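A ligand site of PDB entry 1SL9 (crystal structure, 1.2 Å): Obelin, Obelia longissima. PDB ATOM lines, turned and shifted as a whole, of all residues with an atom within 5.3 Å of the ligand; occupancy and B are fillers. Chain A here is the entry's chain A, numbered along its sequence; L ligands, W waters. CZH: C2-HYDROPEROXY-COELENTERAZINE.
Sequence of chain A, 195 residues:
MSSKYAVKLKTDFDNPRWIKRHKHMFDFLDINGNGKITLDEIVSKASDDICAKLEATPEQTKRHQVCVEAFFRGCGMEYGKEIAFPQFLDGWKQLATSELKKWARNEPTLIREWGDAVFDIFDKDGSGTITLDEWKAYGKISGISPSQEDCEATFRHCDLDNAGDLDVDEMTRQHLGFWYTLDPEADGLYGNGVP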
ATOM      1  N   HIS A  22       3.929  27.023 -26.551  1.00  0.00           N
ATOM      2  CA  HIS A  22       4.870  26.433 -27.550  1.00  0.00           C
ATOM      3  C   HIS A  22       5.063  27.324 -28.732  1.00  0.00           C
ATOM      4  O   HIS A  22       6.155  27.278 -29.334  1.00  0.00           O
ATOM      5  CB  HIS A  22       4.341  25.022 -27.891  1.00  0.00           C
ATOM      6  CG  HIS A  22       4.635  24.088 -26.764  1.00  0.00           C
ATOM      7  ND1 HIS A  22       5.934  23.732 -26.487  1.00  0.00           N
ATOM      8  CD2 HIS A  22       3.772  23.536 -25.899  1.00  0.00           C
ATOM      9  CE1 HIS A  22       5.868  22.920 -25.415  1.00  0.00           C
ATOM     10  NE2 HIS A  22       4.557  22.787 -25.030  1.00  0.00           N
ATOM     11  N   MET A  25       7.769  29.590 -27.857  1.00  0.00           N
ATOM     12  CA  MET A  25       9.072  28.874 -27.917  1.00  0.00           C
ATOM     13  C   MET A  25       9.516  28.623 -29.354  1.00  0.00           C
ATOM     14  O   MET A  25      10.695  28.848 -29.659  1.00  0.00           O
ATOM     15  CB  MET A  25       9.045  27.602 -27.136  1.00  0.00           C
ATOM     16  CG  MET A  25       8.913  27.799 -25.612  1.00  0.00           C
ATOM     17  SD  MET A  25      10.122  28.897 -24.882  1.00  0.00           S
ATOM     18  CE  MET A  25      11.644  28.007 -25.247  1.00  0.00           C
ATOM     19  N   PHE A  26       8.579  28.216 -30.201  1.00  0.00           N
ATOM     20  CA  PHE A  26       8.925  27.997 -31.580  1.00  0.00           C
ATOM     21  C   PHE A  26       9.480  29.289 -32.156  1.00  0.00           C
ATOM     22  O   PHE A  26      10.487  29.308 -32.873  1.00  0.00           O
ATOM     23  CB  PHE A  26       7.688  27.487 -32.314  1.00  0.00           C
ATOM     24  CG  PHE A  26       7.989  27.202 -33.772  1.00  0.00           C
ATOM     25  CD1 PHE A  26       8.311  25.927 -34.185  1.00  0.00           C
ATOM     26  CD2 PHE A  26       7.933  28.170 -34.735  1.00  0.00           C
ATOM     27  CE1 PHE A  26       8.600  25.689 -35.506  1.00  0.00           C
ATOM     28  CE2 PHE A  26       8.277  27.942 -36.041  1.00  0.00           C
ATOM     29  CZ  PHE A  26       8.622  26.678 -36.419  1.00  0.00           C
ATOM     30  N   PHE A  28      10.746  31.827 -30.776  1.00  0.00           N
ATOM     31  CA  PHE A  28      12.049  32.096 -30.195  1.00  0.00           C
ATOM     32  C   PHE A  28      13.145  31.288 -30.853  1.00  0.00           C
ATOM     33  O   PHE A  28      14.231  31.826 -31.063  1.00  0.00           O
ATOM     34  CB  PHE A  28      11.927  31.779 -28.694  1.00  0.00           C
ATOM     35  CG  PHE A  28      13.186  31.490 -27.958  1.00  0.00           C
ATOM     36  CD1 PHE A  28      14.059  32.473 -27.593  1.00  0.00           C
ATOM     37  CD2 PHE A  28      13.479  30.190 -27.585  1.00  0.00           C
ATOM     38  CE1 PHE A  28      15.191  32.204 -26.892  1.00  0.00           C
ATOM     39  CE2 PHE A  28      14.609  29.904 -26.894  1.00  0.00           C
ATOM     40  CZ  PHE A  28      15.511  30.897 -26.531  1.00  0.00           C
ATOM     41  N   LEU A  29      12.874  30.032 -31.176  1.00  0.00           N
ATOM     42  CA  LEU A  29      13.837  29.226 -31.895  1.00  0.00           C
ATOM     43  C   LEU A  29      13.995  29.606 -33.351  1.00  0.00           C
ATOM     44  O   LEU A  29      15.062  29.360 -33.908  1.00  0.00           O
ATOM     45  CB  LEU A  29      13.476  27.754 -31.749  1.00  0.00           C
ATOM     46  CG  LEU A  29      13.563  27.217 -30.320  1.00  0.00           C
ATOM     47  CD1 LEU A  29      12.966  25.840 -30.240  1.00  0.00           C
ATOM     48  CD2 LEU A  29      14.994  27.204 -29.834  1.00  0.00           C
ATOM     49  N   ILE A  42      18.816  23.407 -33.292  1.00  0.00           N
ATOM     50  CA  ILE A  42      18.553  23.201 -31.877  1.00  0.00           C
ATOM     51  C   ILE A  42      19.801  22.631 -31.236  1.00  0.00           C
ATOM     52  O   ILE A  42      20.204  23.050 -30.158  1.00  0.00           O
ATOM     53  CB  ILE A  42      17.293  22.384 -31.685  1.00  0.00           C
ATOM     54  CG1 ILE A  42      16.027  23.264 -31.749  1.00  0.00           C
ATOM     55  CG2 ILE A  42      17.322  21.589 -30.382  1.00  0.00           C
ATOM     56  CD1 ILE A  42      15.929  24.285 -32.855  1.00  0.00           C
ATOM     57  N   LYS A  45      22.533  25.246 -30.986  1.00  0.00           N
ATOM     58  CA  LYS A  45      22.244  26.136 -29.877  1.00  0.00           C
ATOM     59  C   LYS A  45      22.667  25.470 -28.570  1.00  0.00           C
ATOM     60  O   LYS A  45      23.310  26.081 -27.730  1.00  0.00           O
ATOM     61  CB  LYS A  45      20.762  26.480 -29.874  1.00  0.00           C
ATOM     62  CG  LYS A  45      20.291  27.356 -28.735  1.00  0.00           C
ATOM     63  CD  LYS A  45      18.787  27.617 -28.845  1.00  0.00           C
ATOM     64  CE  LYS A  45      18.256  28.480 -27.715  1.00  0.00           C
ATOM     65  NZ  LYS A  45      18.798  29.874 -27.835  1.00  0.00           N
ATOM     66  N   ALA A  46      22.321  24.196 -28.425  1.00  0.00           N
ATOM     67  CA  ALA A  46      22.690  23.445 -27.242  1.00  0.00           C
ATOM     68  C   ALA A  46      24.186  23.348 -27.035  1.00  0.00           C
ATOM     69  O   ALA A  46      24.698  23.592 -25.953  1.00  0.00           O
ATOM     70  CB  ALA A  46      22.076  22.054 -27.312  1.00  0.00           C
ATOM     71  N   ILE A  50      25.217  27.259 -25.922  1.00  0.00           N
ATOM     72  CA  ILE A  50      24.972  27.146 -24.471  1.00  0.00           C
ATOM     73  C   ILE A  50      26.104  26.408 -23.787  1.00  0.00           C
ATOM     74  O   ILE A  50      26.678  26.938 -22.839  1.00  0.00           O
ATOM     75  CB  ILE A  50      23.630  26.462 -24.274  1.00  0.00           C
ATOM     76  CG1 ILE A  50      22.477  27.354 -24.744  1.00  0.00           C
ATOM     77  CG2 ILE A  50      23.458  26.040 -22.824  1.00  0.00           C
ATOM     78  CD1 ILE A  50      21.140  26.669 -24.781  1.00  0.00           C
ATOM     79  N   HIS A  64      24.858  16.238 -22.811  1.00  0.00           N
ATOM     80  CA  HIS A  64      23.742  17.191 -23.038  1.00  0.00           C
ATOM     81  C   HIS A  64      23.251  17.095 -24.447  1.00  0.00           C
ATOM     82  O   HIS A  64      22.032  17.110 -24.712  1.00  0.00           O
ATOM     83  CB  HIS A  64      24.273  18.587 -22.690  1.00  0.00           C
ATOM     84  CG  HIS A  64      23.266  19.677 -22.770  1.00  0.00           C
ATOM     85  ND1 HIS A  64      23.142  20.469 -23.899  1.00  0.00           N
ATOM     86  CD2 HIS A  64      22.359  20.120 -21.881  1.00  0.00           C
ATOM     87  CE1 HIS A  64      22.186  21.368 -23.667  1.00  0.00           C
ATOM     88  NE2 HIS A  64      21.714  21.176 -22.463  1.00  0.00           N
ATOM     89  N   VAL A  68      19.407  16.413 -25.682  1.00  0.00           N
ATOM     90  CA  VAL A  68      18.659  17.365 -26.522  1.00  0.00           C
ATOM     91  C   VAL A  68      18.180  16.679 -27.769  1.00  0.00           C
ATOM     92  O   VAL A  68      17.060  16.848 -28.226  1.00  0.00           O
ATOM     93  CB  VAL A  68      19.552  18.592 -26.802  1.00  0.00           C
ATOM     94  CG1 VAL A  68      18.999  19.460 -27.900  1.00  0.00           C
ATOM     95  CG2 VAL A  68      19.783  19.373 -25.524  1.00  0.00           C
ATOM     96  N   PHE A  72      14.155  16.419 -28.591  1.00  0.00           N
ATOM     97  CA  PHE A  72      13.548  17.042 -29.739  1.00  0.00           C
ATOM     98  C   PHE A  72      13.185  16.051 -30.824  1.00  0.00           C
ATOM     99  O   PHE A  72      12.231  16.238 -31.571  1.00  0.00           O
ATOM    100  CB  PHE A  72      14.428  18.214 -30.257  1.00  0.00           C
ATOM    101  CG  PHE A  72      14.308  19.421 -29.311  1.00  0.00           C
ATOM    102  CD1 PHE A  72      15.272  19.665 -28.350  1.00  0.00           C
ATOM    103  CD2 PHE A  72      13.175  20.238 -29.386  1.00  0.00           C
ATOM    104  CE1 PHE A  72      15.114  20.752 -27.469  1.00  0.00           C
ATOM    105  CE2 PHE A  72      13.059  21.286 -28.524  1.00  0.00           C
ATOM    106  CZ  PHE A  72      13.991  21.530 -27.519  1.00  0.00           C
ATOM    107  N   PHE A  88       5.408  20.838 -35.471  1.00  0.00           N
ATOM    108  CA  PHE A  88       6.123  20.902 -34.194  1.00  0.00           C
ATOM    109  C   PHE A  88       5.197  20.698 -33.023  1.00  0.00           C
ATOM    110  O   PHE A  88       5.488  19.920 -32.117  1.00  0.00           O
ATOM    111  CB  PHE A  88       6.825  22.237 -34.082  1.00  0.00           C
ATOM    112  CG  PHE A  88       7.680  22.524 -32.906  1.00  0.00           C
ATOM    113  CD1 PHE A  88       8.934  21.941 -32.808  1.00  0.00           C
ATOM    114  CD2 PHE A  88       7.265  23.429 -31.939  1.00  0.00           C
ATOM    115  CE1 PHE A  88       9.782  22.267 -31.735  1.00  0.00           C
ATOM    116  CE2 PHE A  88       8.070  23.712 -30.905  1.00  0.00           C
ATOM    117  CZ  PHE A  88       9.337  23.171 -30.802  1.00  0.00           C
ATOM    118  N   TRP A  92       4.945  17.782 -30.092  1.00  0.00           N
ATOM    119  CA  TRP A  92       4.855  18.014 -28.654  1.00  0.00           C
ATOM    120  C   TRP A  92       3.694  17.209 -28.045  1.00  0.00           C
ATOM    121  O   TRP A  92       3.881  16.742 -26.921  1.00  0.00           O
ATOM    122  CB  TRP A  92       4.710  19.507 -28.374  1.00  0.00           C
ATOM    123  CG  TRP A  92       6.048  20.146 -28.202  1.00  0.00           C
ATOM    124  CD1 TRP A  92       6.764  20.778 -29.162  1.00  0.00           C
ATOM    125  CD2 TRP A  92       6.809  20.196 -27.007  1.00  0.00           C
ATOM    126  NE1 TRP A  92       7.928  21.224 -28.644  1.00  0.00           N
ATOM    127  CE2 TRP A  92       7.993  20.888 -27.332  1.00  0.00           C
ATOM    128  CE3 TRP A  92       6.624  19.738 -25.730  1.00  0.00           C
ATOM    129  CZ2 TRP A  92       8.963  21.103 -26.382  1.00  0.00           C
ATOM    130  CZ3 TRP A  92       7.625  19.984 -24.797  1.00  0.00           C
ATOM    131  CH2 TRP A  92       8.781  20.666 -25.119  1.00  0.00           C
ATOM    132  N   ILE A 111      12.604  14.846 -20.387  1.00  0.00           N
ATOM    133  CA  ILE A 111      12.802  16.192 -19.813  1.00  0.00           C
ATOM    134  C   ILE A 111      13.616  16.067 -18.546  1.00  0.00           C
ATOM    135  O   ILE A 111      14.400  16.944 -18.246  1.00  0.00           O
ATOM    136  CB  ILE A 111      11.457  16.919 -19.629  1.00  0.00           C
ATOM    137  CG1 ILE A 111      11.644  18.386 -19.235  1.00  0.00           C
ATOM    138  CG2 ILE A 111      10.491  16.248 -18.687  1.00  0.00           C
ATOM    139  CD1 ILE A 111      12.494  19.264 -20.117  1.00  0.00           C
ATOM    140  N   TRP A 114      17.316  15.528 -19.760  1.00  0.00           N
ATOM    141  CA  TRP A 114      17.850  16.821 -20.139  1.00  0.00           C
ATOM    142  C   TRP A 114      18.176  17.645 -18.906  1.00  0.00           C
ATOM    143  O   TRP A 114      19.288  18.198 -18.814  1.00  0.00           O
ATOM    144  CB  TRP A 114      16.819  17.522 -21.067  1.00  0.00           C
ATOM    145  CG  TRP A 114      17.381  18.738 -21.693  1.00  0.00           C
ATOM    146  CD1 TRP A 114      18.655  19.222 -21.701  1.00  0.00           C
ATOM    147  CD2 TRP A 114      16.599  19.678 -22.469  1.00  0.00           C
ATOM    148  NE1 TRP A 114      18.716  20.390 -22.411  1.00  0.00           N
ATOM    149  CE2 TRP A 114      17.492  20.688 -22.894  1.00  0.00           C
ATOM    150  CE3 TRP A 114      15.267  19.755 -22.842  1.00  0.00           C
ATOM    151  CZ2 TRP A 114      17.082  21.758 -23.668  1.00  0.00           C
ATOM    152  CZ3 TRP A 114      14.874  20.819 -23.608  1.00  0.00           C
ATOM    153  CH2 TRP A 114      15.760  21.805 -24.011  1.00  0.00           C
ATOM    154  N   GLY A 115      17.286  17.724 -17.940  1.00  0.00           N
ATOM    155  CA  GLY A 115      17.593  18.434 -16.729  1.00  0.00           C
ATOM    156  C   GLY A 115      18.852  17.901 -16.033  1.00  0.00           C
ATOM    157  O   GLY A 115      19.678  18.655 -15.573  1.00  0.00           O
ATOM    158  N   VAL A 118      21.783  19.339 -17.768  1.00  0.00           N
ATOM    159  CA  VAL A 118      21.956  20.758 -17.528  1.00  0.00           C
ATOM    160  C   VAL A 118      22.481  20.990 -16.114  1.00  0.00           C
ATOM    161  O   VAL A 118      23.429  21.737 -15.893  1.00  0.00           O
ATOM    162  CB  VAL A 118      20.639  21.543 -17.756  1.00  0.00           C
ATOM    163  CG1 VAL A 118      20.814  22.992 -17.352  1.00  0.00           C
ATOM    164  CG2 VAL A 118      20.229  21.485 -19.183  1.00  0.00           C
ATOM    165  N   PHE A 119      21.851  20.306 -15.178  1.00  0.00           N
ATOM    166  CA  PHE A 119      22.233  20.486 -13.796  1.00  0.00           C
ATOM    167  C   PHE A 119      23.676  20.069 -13.574  1.00  0.00           C
ATOM    168  O   PHE A 119      24.394  20.660 -12.787  1.00  0.00           O
ATOM    169  CB  PHE A 119      21.330  19.677 -12.846  1.00  0.00           C
ATOM    170  CG  PHE A 119      20.056  20.435 -12.492  1.00  0.00           C
ATOM    171  CD1 PHE A 119      19.144  20.839 -13.409  1.00  0.00           C
ATOM    172  CD2 PHE A 119      19.802  20.713 -11.165  1.00  0.00           C
ATOM    173  CE1 PHE A 119      18.016  21.530 -13.021  1.00  0.00           C
ATOM    174  CE2 PHE A 119      18.681  21.393 -10.778  1.00  0.00           C
ATOM    175  CZ  PHE A 119      17.761  21.793 -11.729  1.00  0.00           C
ATOM    176  N   TRP A 135      20.810  29.747 -12.494  1.00  0.00           N
ATOM    177  CA  TRP A 135      19.622  29.817 -13.303  1.00  0.00           C
ATOM    178  C   TRP A 135      19.570  31.153 -14.063  1.00  0.00           C
ATOM    179  O   TRP A 135      19.185  31.190 -15.223  1.00  0.00           O
ATOM    180  CB  TRP A 135      18.387  29.605 -12.447  1.00  0.00           C
ATOM    181  CG  TRP A 135      17.123  29.554 -13.240  1.00  0.00           C
ATOM    182  CD1 TRP A 135      16.044  30.371 -13.107  1.00  0.00           C
ATOM    183  CD2 TRP A 135      16.777  28.621 -14.268  1.00  0.00           C
ATOM    184  NE1 TRP A 135      15.065  30.040 -13.980  1.00  0.00           N
ATOM    185  CE2 TRP A 135      15.490  28.966 -14.703  1.00  0.00           C
ATOM    186  CE3 TRP A 135      17.424  27.548 -14.868  1.00  0.00           C
ATOM    187  CZ2 TRP A 135      14.846  28.258 -15.715  1.00  0.00           C
ATOM    188  CZ3 TRP A 135      16.798  26.835 -15.873  1.00  0.00           C
ATOM    189  CH2 TRP A 135      15.526  27.211 -16.266  1.00  0.00           C
ATOM    190  N   TYR A 138      21.774  30.733 -17.003  1.00  0.00           N
ATOM    191  CA  TYR A 138      21.115  29.874 -17.976  1.00  0.00           C
ATOM    192  C   TYR A 138      20.082  30.686 -18.738  1.00  0.00           C
ATOM    193  O   TYR A 138      19.950  30.582 -19.951  1.00  0.00           O
ATOM    194  CB  TYR A 138      20.462  28.619 -17.312  1.00  0.00           C
ATOM    195  CG  TYR A 138      19.925  27.774 -18.460  1.00  0.00           C
ATOM    196  CD1 TYR A 138      20.807  26.973 -19.177  1.00  0.00           C
ATOM    197  CD2 TYR A 138      18.568  27.789 -18.804  1.00  0.00           C
ATOM    198  CE1 TYR A 138      20.368  26.184 -20.217  1.00  0.00           C
ATOM    199  CE2 TYR A 138      18.150  27.033 -19.863  1.00  0.00           C
ATOM    200  CZ  TYR A 138      19.027  26.228 -20.573  1.00  0.00           C
ATOM    201  OH  TYR A 138      18.580  25.503 -21.622  1.00  0.00           O
ATOM    202  N   SER A 142      20.830  30.651 -22.665  1.00  0.00           N
ATOM    203  CA  SER A 142      19.856  29.962 -23.505  1.00  0.00           C
ATOM    204  C   SER A 142      18.925  30.960 -24.165  1.00  0.00           C
ATOM    205  O   SER A 142      18.369  30.655 -25.177  1.00  0.00           O
ATOM    206  CB  SER A 142      19.041  28.959 -22.694  1.00  0.00           C
ATOM    207  OG  SER A 142      18.102  29.612 -21.897  1.00  0.00           O
ATOM    208  N   ILE A 144      16.120  31.806 -22.885  1.00  0.00           N
ATOM    209  CA  ILE A 144      14.707  31.527 -22.594  1.00  0.00           C
ATOM    210  C   ILE A 144      14.173  32.519 -21.580  1.00  0.00           C
ATOM    211  O   ILE A 144      12.970  32.773 -21.546  1.00  0.00           O
ATOM    212  CB  ILE A 144      14.544  30.097 -22.095  1.00  0.00           C
ATOM    213  CG1 ILE A 144      13.089  29.667 -22.152  1.00  0.00           C
ATOM    214  CG2 ILE A 144      15.126  29.871 -20.708  1.00  0.00           C
ATOM    215  CD1 ILE A 144      12.867  28.175 -22.069  1.00  0.00           C
ATOM    216  N   MET A 171      12.350  20.679 -10.483  1.00  0.00           N
ATOM    217  CA  MET A 171      12.228  21.343 -11.788  1.00  0.00           C
ATOM    218  C   MET A 171      11.531  20.454 -12.803  1.00  0.00           C
ATOM    219  O   MET A 171      10.819  20.938 -13.687  1.00  0.00           O
ATOM    220  CB  MET A 171      13.616  21.794 -12.265  1.00  0.00           C
ATOM    221  CG  MET A 171      13.595  22.697 -13.477  1.00  0.00           C
ATOM    222  SD  MET A 171      12.481  24.087 -13.320  1.00  0.00           S
ATOM    223  CE  MET A 171      13.312  25.174 -14.470  1.00  0.00           C
ATOM    224  N   HIS A 175       8.395  21.183 -14.948  1.00  0.00           N
ATOM    225  CA  HIS A 175       8.392  21.096 -16.422  1.00  0.00           C
ATOM    226  C   HIS A 175       7.399  20.129 -16.991  1.00  0.00           C
ATOM    227  O   HIS A 175       6.903  20.433 -18.054  1.00  0.00           O
ATOM    228  CB  HIS A 175       9.815  20.603 -16.889  1.00  0.00           C
ATOM    229  CG  HIS A 175      10.759  21.701 -16.981  1.00  0.00           C
ATOM    230  ND1 HIS A 175      12.206  21.438 -16.897  1.00  0.00           N
ATOM    231  CD2 HIS A 175      10.564  23.074 -17.235  1.00  0.00           C
ATOM    232  CE1 HIS A 175      12.729  22.648 -17.196  1.00  0.00           C
ATOM    233  NE2 HIS A 175      11.810  23.643 -17.440  1.00  0.00           N
ATOM    234  N   TRP A 179       5.407  22.258 -19.644  1.00  0.00           N
ATOM    235  CA  TRP A 179       5.523  21.972 -21.055  1.00  0.00           C
ATOM    236  C   TRP A 179       4.487  20.952 -21.549  1.00  0.00           C
ATOM    237  O   TRP A 179       4.132  21.053 -22.721  1.00  0.00           O
ATOM    238  CB  TRP A 179       6.889  21.472 -21.404  1.00  0.00           C
ATOM    239  CG  TRP A 179       8.043  22.413 -21.125  1.00  0.00           C
ATOM    240  CD1 TRP A 179       9.148  22.114 -20.391  1.00  0.00           C
ATOM    241  CD2 TRP A 179       8.187  23.750 -21.583  1.00  0.00           C
ATOM    242  NE1 TRP A 179      10.009  23.169 -20.339  1.00  0.00           N
ATOM    243  CE2 TRP A 179       9.437  24.203 -21.069  1.00  0.00           C
ATOM    244  CE3 TRP A 179       7.425  24.626 -22.353  1.00  0.00           C
ATOM    245  CZ2 TRP A 179       9.908  25.494 -21.319  1.00  0.00           C
ATOM    246  CZ3 TRP A 179       7.902  25.877 -22.596  1.00  0.00           C
ATOM    247  CH2 TRP A 179       9.127  26.303 -22.074  1.00  0.00           C
ATOM    248  N   TYR A 190       8.522  30.339 -15.520  1.00  0.00           N
ATOM    249  CA  TYR A 190       9.546  31.173 -16.137  1.00  0.00           C
ATOM    250  C   TYR A 190       9.170  32.623 -15.970  1.00  0.00           C
ATOM    251  O   TYR A 190       9.569  33.460 -16.739  1.00  0.00           O
ATOM    252  CB  TYR A 190       9.743  30.820 -17.623  1.00  0.00           C
ATOM    253  CG  TYR A 190      10.405  29.482 -17.843  1.00  0.00           C
ATOM    254  CD1 TYR A 190       9.715  28.289 -17.843  1.00  0.00           C
ATOM    255  CD2 TYR A 190      11.799  29.484 -18.059  1.00  0.00           C
ATOM    256  CE1 TYR A 190      10.393  27.123 -18.038  1.00  0.00           C
ATOM    257  CE2 TYR A 190      12.460  28.279 -18.247  1.00  0.00           C
ATOM    258  CZ  TYR A 190      11.762  27.107 -18.241  1.00  0.00           C
ATOM    259  OH  TYR A 190      12.486  25.939 -18.460  1.00  0.00           O
HETATM  260  N1  CZH L   1      15.916  24.916 -21.754  1.00  0.00           N
HETATM  261  C2  CZH L   1      15.556  24.212 -20.568  1.00  0.00           C
HETATM  262  C3  CZH L   1      14.049  23.786 -20.935  1.00  0.00           C
HETATM  263  N4  CZH L   1      13.860  24.101 -22.196  1.00  0.00           N
HETATM  264  C5  CZH L   1      12.715  23.919 -23.020  1.00  0.00           C
HETATM  265  C6  CZH L   1      12.747  24.520 -24.282  1.00  0.00           C
HETATM  266  N7  CZH L   1      13.783  25.246 -24.661  1.00  0.00           N
HETATM  267  C8  CZH L   1      14.811  25.444 -23.946  1.00  0.00           C
HETATM  268  C9  CZH L   1      14.936  24.845 -22.670  1.00  0.00           C
HETATM  269  C10 CZH L   1      16.546  23.230 -20.217  1.00  0.00           C
HETATM  270  C11 CZH L   1      16.271  22.502 -19.081  1.00  0.00           C
HETATM  271  C12 CZH L   1      16.509  23.124 -17.793  1.00  0.00           C
HETATM  272  C13 CZH L   1      16.269  22.335 -16.481  1.00  0.00           C
HETATM  273  C14 CZH L   1      15.623  21.145 -16.649  1.00  0.00           C
HETATM  274  C15 CZH L   1      15.331  20.544 -17.830  1.00  0.00           C
HETATM  275  C16 CZH L   1      15.660  21.224 -18.970  1.00  0.00           C
HETATM  276  O18 CZH L   1      13.278  23.143 -20.361  1.00  0.00           O
HETATM  277  C19 CZH L   1      11.607  24.425 -25.174  1.00  0.00           C
HETATM  278  C20 CZH L   1      11.792  24.547 -26.514  1.00  0.00           C
HETATM  279  C21 CZH L   1      10.671  24.557 -27.389  1.00  0.00           C
HETATM  280  C22 CZH L   1       9.352  24.334 -26.834  1.00  0.00           C
HETATM  281  C23 CZH L   1       9.205  24.236 -25.481  1.00  0.00           C
HETATM  282  C24 CZH L   1      10.311  24.247 -24.658  1.00  0.00           C
HETATM  283  O25 CZH L   1       8.306  24.325 -27.709  1.00  0.00           O
HETATM  284  C26 CZH L   1      15.989  26.319 -24.438  1.00  0.00           C
HETATM  285  C27 CZH L   1      16.786  25.454 -25.445  1.00  0.00           C
HETATM  286  C28 CZH L   1      18.067  25.007 -25.150  1.00  0.00           C
HETATM  287  C29 CZH L   1      18.824  24.268 -26.050  1.00  0.00           C
HETATM  288  C30 CZH L   1      18.295  24.004 -27.233  1.00  0.00           C
HETATM  289  C31 CZH L   1      17.051  24.441 -27.614  1.00  0.00           C
HETATM  290  C32 CZH L   1      16.278  25.224 -26.649  1.00  0.00           C
HETATM  291  O33 CZH L   1      15.423  25.117 -19.506  1.00  0.00           O
HETATM  292  O34 CZH L   1      14.609  26.201 -19.855  1.00  0.00           O
HETATM  293  O   HOH W   1      13.376  18.718 -16.051  1.00  0.00           O
HETATM  294  O   HOH W   2      20.190  23.635 -22.882  1.00  0.00           O
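Water W1 lies within hydrogen-bond range of the backbone carbonyl oxygen (O) of Ile 111 (3.0 Å) and a ring nitrogen (ND1) of His 175 (3.1 Å).
Water W2 lies within hydrogen-bond range of OH of Tyr 138 (2.8 Å) and NE2 of His 64 (2.9 Å).
OH of Tyr 190 is in hydrogen-bond range of O34 of the ligand, at 2.6 Å.
The side-chain hydroxyl of Tyr 138 lies within hydrogen-bond range of a nitrogen (N1) of the ligand, at 2.7 Å.
O25 of the ligand is in hydrogen-bond range of ND1 of His 22 (2.7 Å).
NE2 of His 175 lies close to O18 of the ligand (3.3 Å).
The indole nitrogen (NE1) of Trp 92 sits at hydrogen-bond distance from an oxygen (O25) of the ligand (3.3 Å).
The indole nitrogen of Trp 179 is in hydrogen-bond range of an oxygen (O18) of the ligand, 3.3 Å away.
Met 25 touches the ligand.
Leu 29 touches the ligand (CD1 to C21, 3.9 Å).
Ile 42 touches the ligand (O to C30, 3.6 Å).
Lys 45 touches the ligand.
Ile 50 touches the ligand.
CZ of Phe 72 touches C20 of the ligand (3.9 Å).
CE2 of Phe 88 touches O25 of the ligand, 3.3 Å away.
Ile 111 touches the ligand (O to C15, 3.7 Å).
CH2 of Trp 114 touches C9 of the ligand (3.4 Å).
Gly 115 touches the ligand.
Phe 119 touches the ligand.
Trp 135 touches the ligand (CH2 to O34, 3.8 Å).
CD1 of Ile 144 touches O34 of the ligand, at 3.4 Å.
Hydrophobic or aromatic side chains that line the ligand: His 22, Met 25, Leu 29, Ile 42, Ile 50, Phe 72, Phe 88, Trp 92, Ile 111, Trp 114, Phe 119, Trp 135, Tyr 138, Ile 144, His 175, Trp 179 and Tyr 190.
Within 4 Å of the ligand: His 22, Met 25, Leu 29, Ile 42, Lys 45, Ile 50, Phe 72, Phe 88, Trp 92, Ile 111, Trp 114, Gly 115, Phe 119, Trp 135, Tyr 138, Ile 144, His 175, Trp 179 and Tyr 190.
NE2 of His 175 sits at hydrogen-bond distance from OH of Tyr 190 (2.6 Å).
The side-chain hydroxyl (OG) of Ser 142 lies within hydrogen-bond range of the backbone carbonyl oxygen (O) of Tyr 138, 2.9 Å away.
NE2 of His 22 is in hydrogen-bond range of O of Trp 179 (2.9 Å).
A ring nitrogen (NE2) of His 175 lies close to the indole nitrogen of Trp 179, 3.4 Å away.
NE1 of Trp 114 sits at hydrogen-bond distance from NE2 of His 64 (3.1 Å).
N of Ile 144 lies within hydrogen-bond range of OG of Ser 142, at 3.1 Å.
The backbone NH (N) of Ile 50 lies within hydrogen-bond range of the backbone carbonyl oxygen (O) of Lys 45 (2.9 Å).
NZ of Lys 45 is in hydrogen-bond range of O of Ser 142, 2.8 Å away.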
